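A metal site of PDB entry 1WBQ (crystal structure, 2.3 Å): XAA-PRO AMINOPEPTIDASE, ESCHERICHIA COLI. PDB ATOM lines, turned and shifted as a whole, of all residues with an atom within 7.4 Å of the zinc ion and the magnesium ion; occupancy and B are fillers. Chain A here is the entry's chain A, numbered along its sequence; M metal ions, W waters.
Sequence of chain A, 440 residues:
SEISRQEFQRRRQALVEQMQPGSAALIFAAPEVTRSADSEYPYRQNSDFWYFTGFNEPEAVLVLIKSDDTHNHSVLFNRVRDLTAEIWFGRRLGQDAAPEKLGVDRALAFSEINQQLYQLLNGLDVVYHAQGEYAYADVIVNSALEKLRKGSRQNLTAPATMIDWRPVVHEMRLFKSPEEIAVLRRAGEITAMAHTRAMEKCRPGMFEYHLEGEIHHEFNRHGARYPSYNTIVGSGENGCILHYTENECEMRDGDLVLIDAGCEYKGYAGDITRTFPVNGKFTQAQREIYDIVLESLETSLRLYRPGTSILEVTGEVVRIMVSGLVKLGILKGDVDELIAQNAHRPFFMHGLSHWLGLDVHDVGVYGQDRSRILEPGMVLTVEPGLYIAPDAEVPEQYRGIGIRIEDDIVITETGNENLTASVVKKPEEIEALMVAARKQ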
ATOM      1  N   TYR A 229       5.786  -7.453   1.083  1.00  0.00           N
ATOM      2  CA  TYR A 229       7.089  -7.179   1.688  1.00  0.00           C
ATOM      3  C   TYR A 229       7.885  -6.351   0.702  1.00  0.00           C
ATOM      4  O   TYR A 229       7.516  -6.251  -0.470  1.00  0.00           O
ATOM      5  CB  TYR A 229       7.829  -8.481   2.012  1.00  0.00           C
ATOM      6  CG  TYR A 229       7.937  -9.414   0.830  1.00  0.00           C
ATOM      7  CD1 TYR A 229       6.898 -10.296   0.525  1.00  0.00           C
ATOM      8  CD2 TYR A 229       9.053  -9.416   0.014  1.00  0.00           C
ATOM      9  CE1 TYR A 229       6.997 -11.177  -0.552  1.00  0.00           C
ATOM     10  CE2 TYR A 229       9.156 -10.265  -1.072  1.00  0.00           C
ATOM     11  CZ  TYR A 229       8.131 -11.151  -1.340  1.00  0.00           C
ATOM     12  OH  TYR A 229       8.237 -12.001  -2.416  1.00  0.00           O
ATOM     13  N   ILE A 232      12.906  -7.271  -3.564  1.00  0.00           N
ATOM     14  CA  ILE A 232      14.342  -7.491  -3.740  1.00  0.00           C
ATOM     15  C   ILE A 232      14.642  -7.669  -5.224  1.00  0.00           C
ATOM     16  O   ILE A 232      14.049  -8.546  -5.888  1.00  0.00           O
ATOM     17  CB  ILE A 232      14.796  -8.775  -2.989  1.00  0.00           C
ATOM     18  CG1 ILE A 232      14.649  -8.609  -1.458  1.00  0.00           C
ATOM     19  CG2 ILE A 232      16.241  -9.176  -3.370  1.00  0.00           C
ATOM     20  CD1 ILE A 232      14.635  -9.928  -0.688  1.00  0.00           C
ATOM     21  N   ILE A 259      15.119 -11.861  -8.224  1.00  0.00           N
ATOM     22  CA  ILE A 259      13.941 -11.040  -7.885  1.00  0.00           C
ATOM     23  C   ILE A 259      13.050 -11.781  -6.918  1.00  0.00           C
ATOM     24  O   ILE A 259      12.511 -12.824  -7.263  1.00  0.00           O
ATOM     25  CB  ILE A 259      13.111 -10.654  -9.128  1.00  0.00           C
ATOM     26  CG1 ILE A 259      14.019  -9.976 -10.162  1.00  0.00           C
ATOM     27  CG2 ILE A 259      11.962  -9.703  -8.733  1.00  0.00           C
ATOM     28  CD1 ILE A 259      13.270  -9.283 -11.256  1.00  0.00           C
ATOM     29  N   ASP A 260      12.919 -11.248  -5.713  1.00  0.00           N
ATOM     30  CA  ASP A 260      11.979 -11.753  -4.735  1.00  0.00           C
ATOM     31  C   ASP A 260      10.904 -10.689  -4.499  1.00  0.00           C
ATOM     32  O   ASP A 260      11.159  -9.643  -3.923  1.00  0.00           O
ATOM     33  CB  ASP A 260      12.684 -12.128  -3.421  1.00  0.00           C
ATOM     34  CG  ASP A 260      11.834 -13.004  -2.515  1.00  0.00           C
ATOM     35  OD1 ASP A 260      10.601 -13.085  -2.730  1.00  0.00           O
ATOM     36  OD2 ASP A 260      12.383 -13.616  -1.583  1.00  0.00           O
ATOM     37  N   ALA A 261       9.691 -10.982  -4.936  1.00  0.00           N
ATOM     38  CA  ALA A 261       8.609 -10.026  -4.847  1.00  0.00           C
ATOM     39  C   ALA A 261       7.275 -10.746  -4.718  1.00  0.00           C
ATOM     40  O   ALA A 261       7.074 -11.821  -5.275  1.00  0.00           O
ATOM     41  CB  ALA A 261       8.607  -9.115  -6.094  1.00  0.00           C
ATOM     42  N   GLY A 262       6.367 -10.118  -3.964  1.00  0.00           N
ATOM     43  CA  GLY A 262       5.043 -10.659  -3.725  1.00  0.00           C
ATOM     44  C   GLY A 262       4.040  -9.563  -3.459  1.00  0.00           C
ATOM     45  O   GLY A 262       4.364  -8.548  -2.827  1.00  0.00           O
ATOM     46  N   GLY A 270       1.441 -13.068  -1.621  1.00  0.00           N
ATOM     47  CA  GLY A 270       2.199 -13.854  -2.569  1.00  0.00           C
ATOM     48  C   GLY A 270       3.673 -13.705  -2.195  1.00  0.00           C
ATOM     49  O   GLY A 270       4.054 -12.732  -1.546  1.00  0.00           O
ATOM     50  N   ASP A 271       4.489 -14.667  -2.611  1.00  0.00           N
ATOM     51  CA  ASP A 271       5.920 -14.660  -2.277  1.00  0.00           C
ATOM     52  C   ASP A 271       6.697 -15.499  -3.281  1.00  0.00           C
ATOM     53  O   ASP A 271       6.856 -16.711  -3.108  1.00  0.00           O
ATOM     54  CB  ASP A 271       6.103 -15.189  -0.848  1.00  0.00           C
ATOM     55  CG  ASP A 271       7.530 -15.090  -0.341  1.00  0.00           C
ATOM     56  OD1 ASP A 271       8.465 -14.604  -1.027  1.00  0.00           O
ATOM     57  OD2 ASP A 271       7.722 -15.507   0.815  1.00  0.00           O
ATOM     58  N   ILE A 272       7.170 -14.846  -4.351  1.00  0.00           N
ATOM     59  CA  ILE A 272       7.884 -15.540  -5.413  1.00  0.00           C
ATOM     60  C   ILE A 272       9.309 -15.011  -5.553  1.00  0.00           C
ATOM     61  O   ILE A 272       9.579 -13.809  -5.432  1.00  0.00           O
ATOM     62  CB  ILE A 272       7.161 -15.390  -6.765  1.00  0.00           C
ATOM     63  CG1 ILE A 272       5.760 -15.998  -6.685  1.00  0.00           C
ATOM     64  CG2 ILE A 272       8.004 -16.053  -7.917  1.00  0.00           C
ATOM     65  CD1 ILE A 272       4.995 -15.982  -8.001  1.00  0.00           C
ATOM     66  N   THR A 273      10.228 -15.942  -5.813  1.00  0.00           N
ATOM     67  CA  THR A 273      11.568 -15.585  -6.239  1.00  0.00           C
ATOM     68  C   THR A 273      11.872 -16.254  -7.569  1.00  0.00           C
ATOM     69  O   THR A 273      11.639 -17.437  -7.746  1.00  0.00           O
ATOM     70  CB  THR A 273      12.667 -15.968  -5.242  1.00  0.00           C
ATOM     71  OG1 THR A 273      12.334 -15.460  -3.949  1.00  0.00           O
ATOM     72  CG2 THR A 273      14.008 -15.370  -5.688  1.00  0.00           C
ATOM     73  N   LEU A 352      14.234 -23.664   4.124  1.00  0.00           N
ATOM     74  CA  LEU A 352      13.668 -24.043   2.841  1.00  0.00           C
ATOM     75  C   LEU A 352      12.248 -23.550   2.682  1.00  0.00           C
ATOM     76  O   LEU A 352      11.801 -23.272   1.569  1.00  0.00           O
ATOM     77  CB  LEU A 352      13.682 -25.572   2.683  1.00  0.00           C
ATOM     78  CG  LEU A 352      13.043 -26.163   1.419  1.00  0.00           C
ATOM     79  CD1 LEU A 352      13.826 -25.763   0.180  1.00  0.00           C
ATOM     80  CD2 LEU A 352      12.950 -27.679   1.531  1.00  0.00           C
ATOM     81  N   SER A 353      11.526 -23.444   3.807  1.00  0.00           N
ATOM     82  CA  SER A 353      10.103 -23.175   3.778  1.00  0.00           C
ATOM     83  C   SER A 353       9.646 -22.377   4.986  1.00  0.00           C
ATOM     84  O   SER A 353      10.084 -22.627   6.095  1.00  0.00           O
ATOM     85  CB  SER A 353       9.334 -24.512   3.742  1.00  0.00           C
ATOM     86  OG  SER A 353       9.588 -25.231   2.535  1.00  0.00           O
ATOM     87  N   HIS A 354       8.740 -21.429   4.779  1.00  0.00           N
ATOM     88  CA  HIS A 354       7.998 -20.806   5.877  1.00  0.00           C
ATOM     89  C   HIS A 354       6.512 -20.828   5.552  1.00  0.00           C
ATOM     90  O   HIS A 354       6.117 -20.920   4.392  1.00  0.00           O
ATOM     91  CB  HIS A 354       8.488 -19.363   6.151  1.00  0.00           C
ATOM     92  CG  HIS A 354       8.390 -18.448   4.965  1.00  0.00           C
ATOM     93  ND1 HIS A 354       7.190 -17.903   4.552  1.00  0.00           N
ATOM     94  CD2 HIS A 354       9.325 -17.996   4.103  1.00  0.00           C
ATOM     95  CE1 HIS A 354       7.396 -17.156   3.487  1.00  0.00           C
ATOM     96  NE2 HIS A 354       8.680 -17.202   3.183  1.00  0.00           N
ATOM     97  N   TRP A 355       5.681 -20.751   6.588  1.00  0.00           N
ATOM     98  CA  TRP A 355       4.237 -20.605   6.403  1.00  0.00           C
ATOM     99  C   TRP A 355       3.945 -19.295   5.667  1.00  0.00           C
ATOM    100  O   TRP A 355       4.739 -18.339   5.720  1.00  0.00           O
ATOM    101  CB  TRP A 355       3.462 -20.548   7.728  1.00  0.00           C
ATOM    102  CG  TRP A 355       3.755 -21.617   8.748  1.00  0.00           C
ATOM    103  CD1 TRP A 355       4.087 -21.426  10.050  1.00  0.00           C
ATOM    104  CD2 TRP A 355       3.685 -23.043   8.568  1.00  0.00           C
ATOM    105  NE1 TRP A 355       4.241 -22.624  10.690  1.00  0.00           N
ATOM    106  CE2 TRP A 355       4.009 -23.642   9.795  1.00  0.00           C
ATOM    107  CE3 TRP A 355       3.380 -23.871   7.473  1.00  0.00           C
ATOM    108  CZ2 TRP A 355       4.055 -25.030   9.984  1.00  0.00           C
ATOM    109  CZ3 TRP A 355       3.421 -25.258   7.653  1.00  0.00           C
ATOM    110  CH2 TRP A 355       3.752 -25.823   8.902  1.00  0.00           C
ATOM    111  N   LEU A 356       2.785 -19.263   5.014  1.00  0.00           N
ATOM    112  CA  LEU A 356       2.385 -18.142   4.215  1.00  0.00           C
ATOM    113  C   LEU A 356       0.907 -17.871   4.423  1.00  0.00           C
ATOM    114  O   LEU A 356       0.100 -18.796   4.465  1.00  0.00           O
ATOM    115  CB  LEU A 356       2.658 -18.443   2.729  1.00  0.00           C
ATOM    116  CG  LEU A 356       2.389 -17.344   1.692  1.00  0.00           C
ATOM    117  CD1 LEU A 356       3.459 -16.250   1.693  1.00  0.00           C
ATOM    118  CD2 LEU A 356       2.275 -17.957   0.306  1.00  0.00           C
ATOM    119  N   VAL A 360       3.602 -12.618   5.322  1.00  0.00           N
ATOM    120  CA  VAL A 360       4.470 -13.358   4.411  1.00  0.00           C
ATOM    121  C   VAL A 360       5.209 -14.456   5.177  1.00  0.00           C
ATOM    122  O   VAL A 360       5.266 -15.595   4.717  1.00  0.00           O
ATOM    123  CB  VAL A 360       5.418 -12.414   3.571  1.00  0.00           C
ATOM    124  CG1 VAL A 360       6.380 -11.626   4.448  1.00  0.00           C
ATOM    125  CG2 VAL A 360       6.199 -13.224   2.537  1.00  0.00           C
ATOM    126  N   HIS A 361       5.769 -14.121   6.339  1.00  0.00           N
ATOM    127  CA  HIS A 361       6.287 -15.144   7.264  1.00  0.00           C
ATOM    128  C   HIS A 361       5.161 -15.368   8.256  1.00  0.00           C
ATOM    129  O   HIS A 361       5.074 -14.697   9.285  1.00  0.00           O
ATOM    130  CB  HIS A 361       7.576 -14.700   7.967  1.00  0.00           C
ATOM    131  CG  HIS A 361       8.715 -14.440   7.038  1.00  0.00           C
ATOM    132  ND1 HIS A 361       9.723 -13.544   7.313  1.00  0.00           N
ATOM    133  CD2 HIS A 361       8.994 -14.934   5.800  1.00  0.00           C
ATOM    134  CE1 HIS A 361      10.573 -13.502   6.293  1.00  0.00           C
ATOM    135  NE2 HIS A 361      10.160 -14.351   5.378  1.00  0.00           N
ATOM    136  N   LEU A 380       2.604 -22.878   2.471  1.00  0.00           N
ATOM    137  CA  LEU A 380       4.003 -22.598   2.725  1.00  0.00           C
ATOM    138  C   LEU A 380       4.767 -22.284   1.453  1.00  0.00           C
ATOM    139  O   LEU A 380       4.291 -22.531   0.353  1.00  0.00           O
ATOM    140  CB  LEU A 380       4.672 -23.776   3.446  1.00  0.00           C
ATOM    141  CG  LEU A 380       4.565 -25.132   2.727  1.00  0.00           C
ATOM    142  CD1 LEU A 380       5.771 -25.982   3.043  1.00  0.00           C
ATOM    143  CD2 LEU A 380       3.251 -25.850   3.064  1.00  0.00           C
ATOM    144  N   THR A 381       5.968 -21.739   1.629  1.00  0.00           N
ATOM    145  CA  THR A 381       6.867 -21.492   0.523  1.00  0.00           C
ATOM    146  C   THR A 381       7.844 -22.652   0.369  1.00  0.00           C
ATOM    147  O   THR A 381       8.024 -23.461   1.286  1.00  0.00           O
ATOM    148  CB  THR A 381       7.649 -20.180   0.703  1.00  0.00           C
ATOM    149  OG1 THR A 381       8.512 -20.274   1.843  1.00  0.00           O
ATOM    150  CG2 THR A 381       6.660 -18.999   0.885  1.00  0.00           C
ATOM    151  N   VAL A 382       8.443 -22.731  -0.813  1.00  0.00           N
ATOM    152  CA  VAL A 382       9.535 -23.655  -1.064  1.00  0.00           C
ATOM    153  C   VAL A 382      10.563 -22.823  -1.795  1.00  0.00           C
ATOM    154  O   VAL A 382      10.311 -22.380  -2.926  1.00  0.00           O
ATOM    155  CB  VAL A 382       9.101 -24.836  -1.961  1.00  0.00           C
ATOM    156  CG1 VAL A 382      10.207 -25.885  -2.036  1.00  0.00           C
ATOM    157  CG2 VAL A 382       7.777 -25.435  -1.446  1.00  0.00           C
ATOM    158  N   GLU A 383      11.715 -22.623  -1.171  1.00  0.00           N
ATOM    159  CA  GLU A 383      12.680 -21.661  -1.692  1.00  0.00           C
ATOM    160  C   GLU A 383      14.141 -22.052  -1.441  1.00  0.00           C
ATOM    161  O   GLU A 383      14.869 -21.359  -0.730  1.00  0.00           O
ATOM    162  CB  GLU A 383      12.383 -20.271  -1.134  1.00  0.00           C
ATOM    163  CG  GLU A 383      12.310 -20.159   0.384  1.00  0.00           C
ATOM    164  CD  GLU A 383      11.911 -18.758   0.842  1.00  0.00           C
ATOM    165  OE1 GLU A 383      12.470 -17.750   0.334  1.00  0.00           O
ATOM    166  OE2 GLU A 383      11.042 -18.668   1.721  1.00  0.00           O
ATOM    167  N   ARG A 404      18.124 -18.023  -6.112  1.00  0.00           N
ATOM    168  CA  ARG A 404      17.023 -18.593  -5.370  1.00  0.00           C
ATOM    169  C   ARG A 404      15.830 -18.750  -6.308  1.00  0.00           C
ATOM    170  O   ARG A 404      15.631 -17.914  -7.194  1.00  0.00           O
ATOM    171  CB  ARG A 404      16.642 -17.733  -4.163  1.00  0.00           C
ATOM    172  CG  ARG A 404      15.471 -18.324  -3.352  1.00  0.00           C
ATOM    173  CD  ARG A 404      15.284 -17.706  -1.997  1.00  0.00           C
ATOM    174  NE  ARG A 404      14.967 -16.264  -2.053  1.00  0.00           N
ATOM    175  CZ  ARG A 404      15.827 -15.267  -1.828  1.00  0.00           C
ATOM    176  NH1 ARG A 404      17.103 -15.501  -1.532  1.00  0.00           N
ATOM    177  NH2 ARG A 404      15.416 -14.014  -1.887  1.00  0.00           N
ATOM    178  N   GLU A 406      11.718 -19.692  -5.801  1.00  0.00           N
ATOM    179  CA  GLU A 406      10.706 -19.848  -4.760  1.00  0.00           C
ATOM    180  C   GLU A 406       9.273 -19.891  -5.302  1.00  0.00           C
ATOM    181  O   GLU A 406       8.824 -18.961  -6.004  1.00  0.00           O
ATOM    182  CB  GLU A 406      10.827 -18.688  -3.775  1.00  0.00           C
ATOM    183  CG  GLU A 406       9.646 -18.533  -2.864  1.00  0.00           C
ATOM    184  CD  GLU A 406       9.856 -17.464  -1.837  1.00  0.00           C
ATOM    185  OE1 GLU A 406      10.552 -16.472  -2.130  1.00  0.00           O
ATOM    186  OE2 GLU A 406       9.307 -17.608  -0.740  1.00  0.00           O
ATOM    187  N   ASP A 407       8.567 -20.959  -4.926  1.00  0.00           N
ATOM    188  CA  ASP A 407       7.141 -21.120  -5.180  1.00  0.00           C
ATOM    189  C   ASP A 407       6.330 -21.149  -3.872  1.00  0.00           C
ATOM    190  O   ASP A 407       6.880 -21.385  -2.784  1.00  0.00           O
ATOM    191  CB  ASP A 407       6.866 -22.403  -5.977  1.00  0.00           C
ATOM    192  CG  ASP A 407       7.154 -22.251  -7.466  1.00  0.00           C
ATOM    193  OD1 ASP A 407       7.042 -21.131  -7.991  1.00  0.00           O
ATOM    194  OD2 ASP A 407       7.450 -23.274  -8.138  1.00  0.00           O
ATOM    195  N   ASP A 408       5.027 -20.915  -4.005  1.00  0.00           N
ATOM    196  CA  ASP A 408       4.080 -21.009  -2.909  1.00  0.00           C
ATOM    197  C   ASP A 408       3.148 -22.187  -3.156  1.00  0.00           C
ATOM    198  O   ASP A 408       2.599 -22.324  -4.260  1.00  0.00           O
ATOM    199  CB  ASP A 408       3.259 -19.724  -2.804  1.00  0.00           C
ATOM    200  CG  ASP A 408       4.114 -18.481  -2.757  1.00  0.00           C
ATOM    201  OD1 ASP A 408       5.257 -18.530  -2.229  1.00  0.00           O
ATOM    202  OD2 ASP A 408       3.641 -17.442  -3.245  1.00  0.00           O
HETATM  203 ZN    ZN M   1       9.519 -16.694   1.199  1.00  0.00          ZN
HETATM  204 MG    MG M   2      10.529 -14.590  -1.114  1.00  0.00          MG
HETATM  205  O   HOH W   1      10.875 -14.319   2.802  1.00  0.00           O
HETATM  206  O   HOH W   2      10.054 -13.023   0.448  1.00  0.00           O
HETATM  207  O   HOH W   3      11.535 -15.514   0.611  1.00  0.00           O
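OE2 of Glu 406 is bound to the zinc ion (2.2 Å). The side-chain carboxylate (OD2) of Asp 271 is bound to the zinc ion (2.2 Å). The zinc ion is bound by a ring nitrogen (NE2) of His 354, 2.2 Å away. Water W3 binds the zinc ion (2.4 Å). The zinc ion is bound by OE2 of Glu 383.
Thr 381 touches the zinc ion. Five residues have an atom within 4 Å of the zinc ion: Asp 271, His 354, Thr 381, Glu 383 and Glu 406.
Tyr 229 touches the magnesium ion. Thr 273 touches the magnesium ion (OG1 to MG, 3.5 Å). Of the 25 residues printed, 6 come within 4 Å of the magnesium ion. The nearest printed residue that does not touch the magnesium ion is Ile 272 (4.5 Å).
The side-chain carboxylate (OD2) of Asp 260 sits close to the guanidinium group (NH2) of Arg 404, 3.1 Å away. The backbone NH of Glu 406 is in hydrogen-bond range of the backbone carbonyl oxygen of Thr 273, at 3.0 Å. The side-chain carboxylate of Asp 260 sits close to the side-chain hydroxyl of Thr 273, 3.0 Å away. The side-chain hydroxyl of Tyr 229 lies close to the backbone NH of Ala 261, 3.1 Å away. OG1 of Thr 273 lies within hydrogen-bond range of NE of Arg 404, 3.3 Å away. OE1 of Glu 383 is in salt-bridge range of NE of Arg 404 (3.8 Å). ND1 of His 354 sits close to O of Val 360, 3.0 Å away. OE2 of Glu 383 sits close to OG1 of Thr 381 (3.0 Å).
The magnesium ion is bound by the side-chain carboxylate (OD1) of Asp 271 (2.1 Å), the side-chain carboxylate (OE1) of Glu 406 (2.1 Å), the side-chain carboxylate (OD2) of Asp 260 (2.1 Å), water W3 (2.2 Å), the side-chain carboxylate (OD1) of Asp 260 (2.2 Å) and water W2 (2.3 Å).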
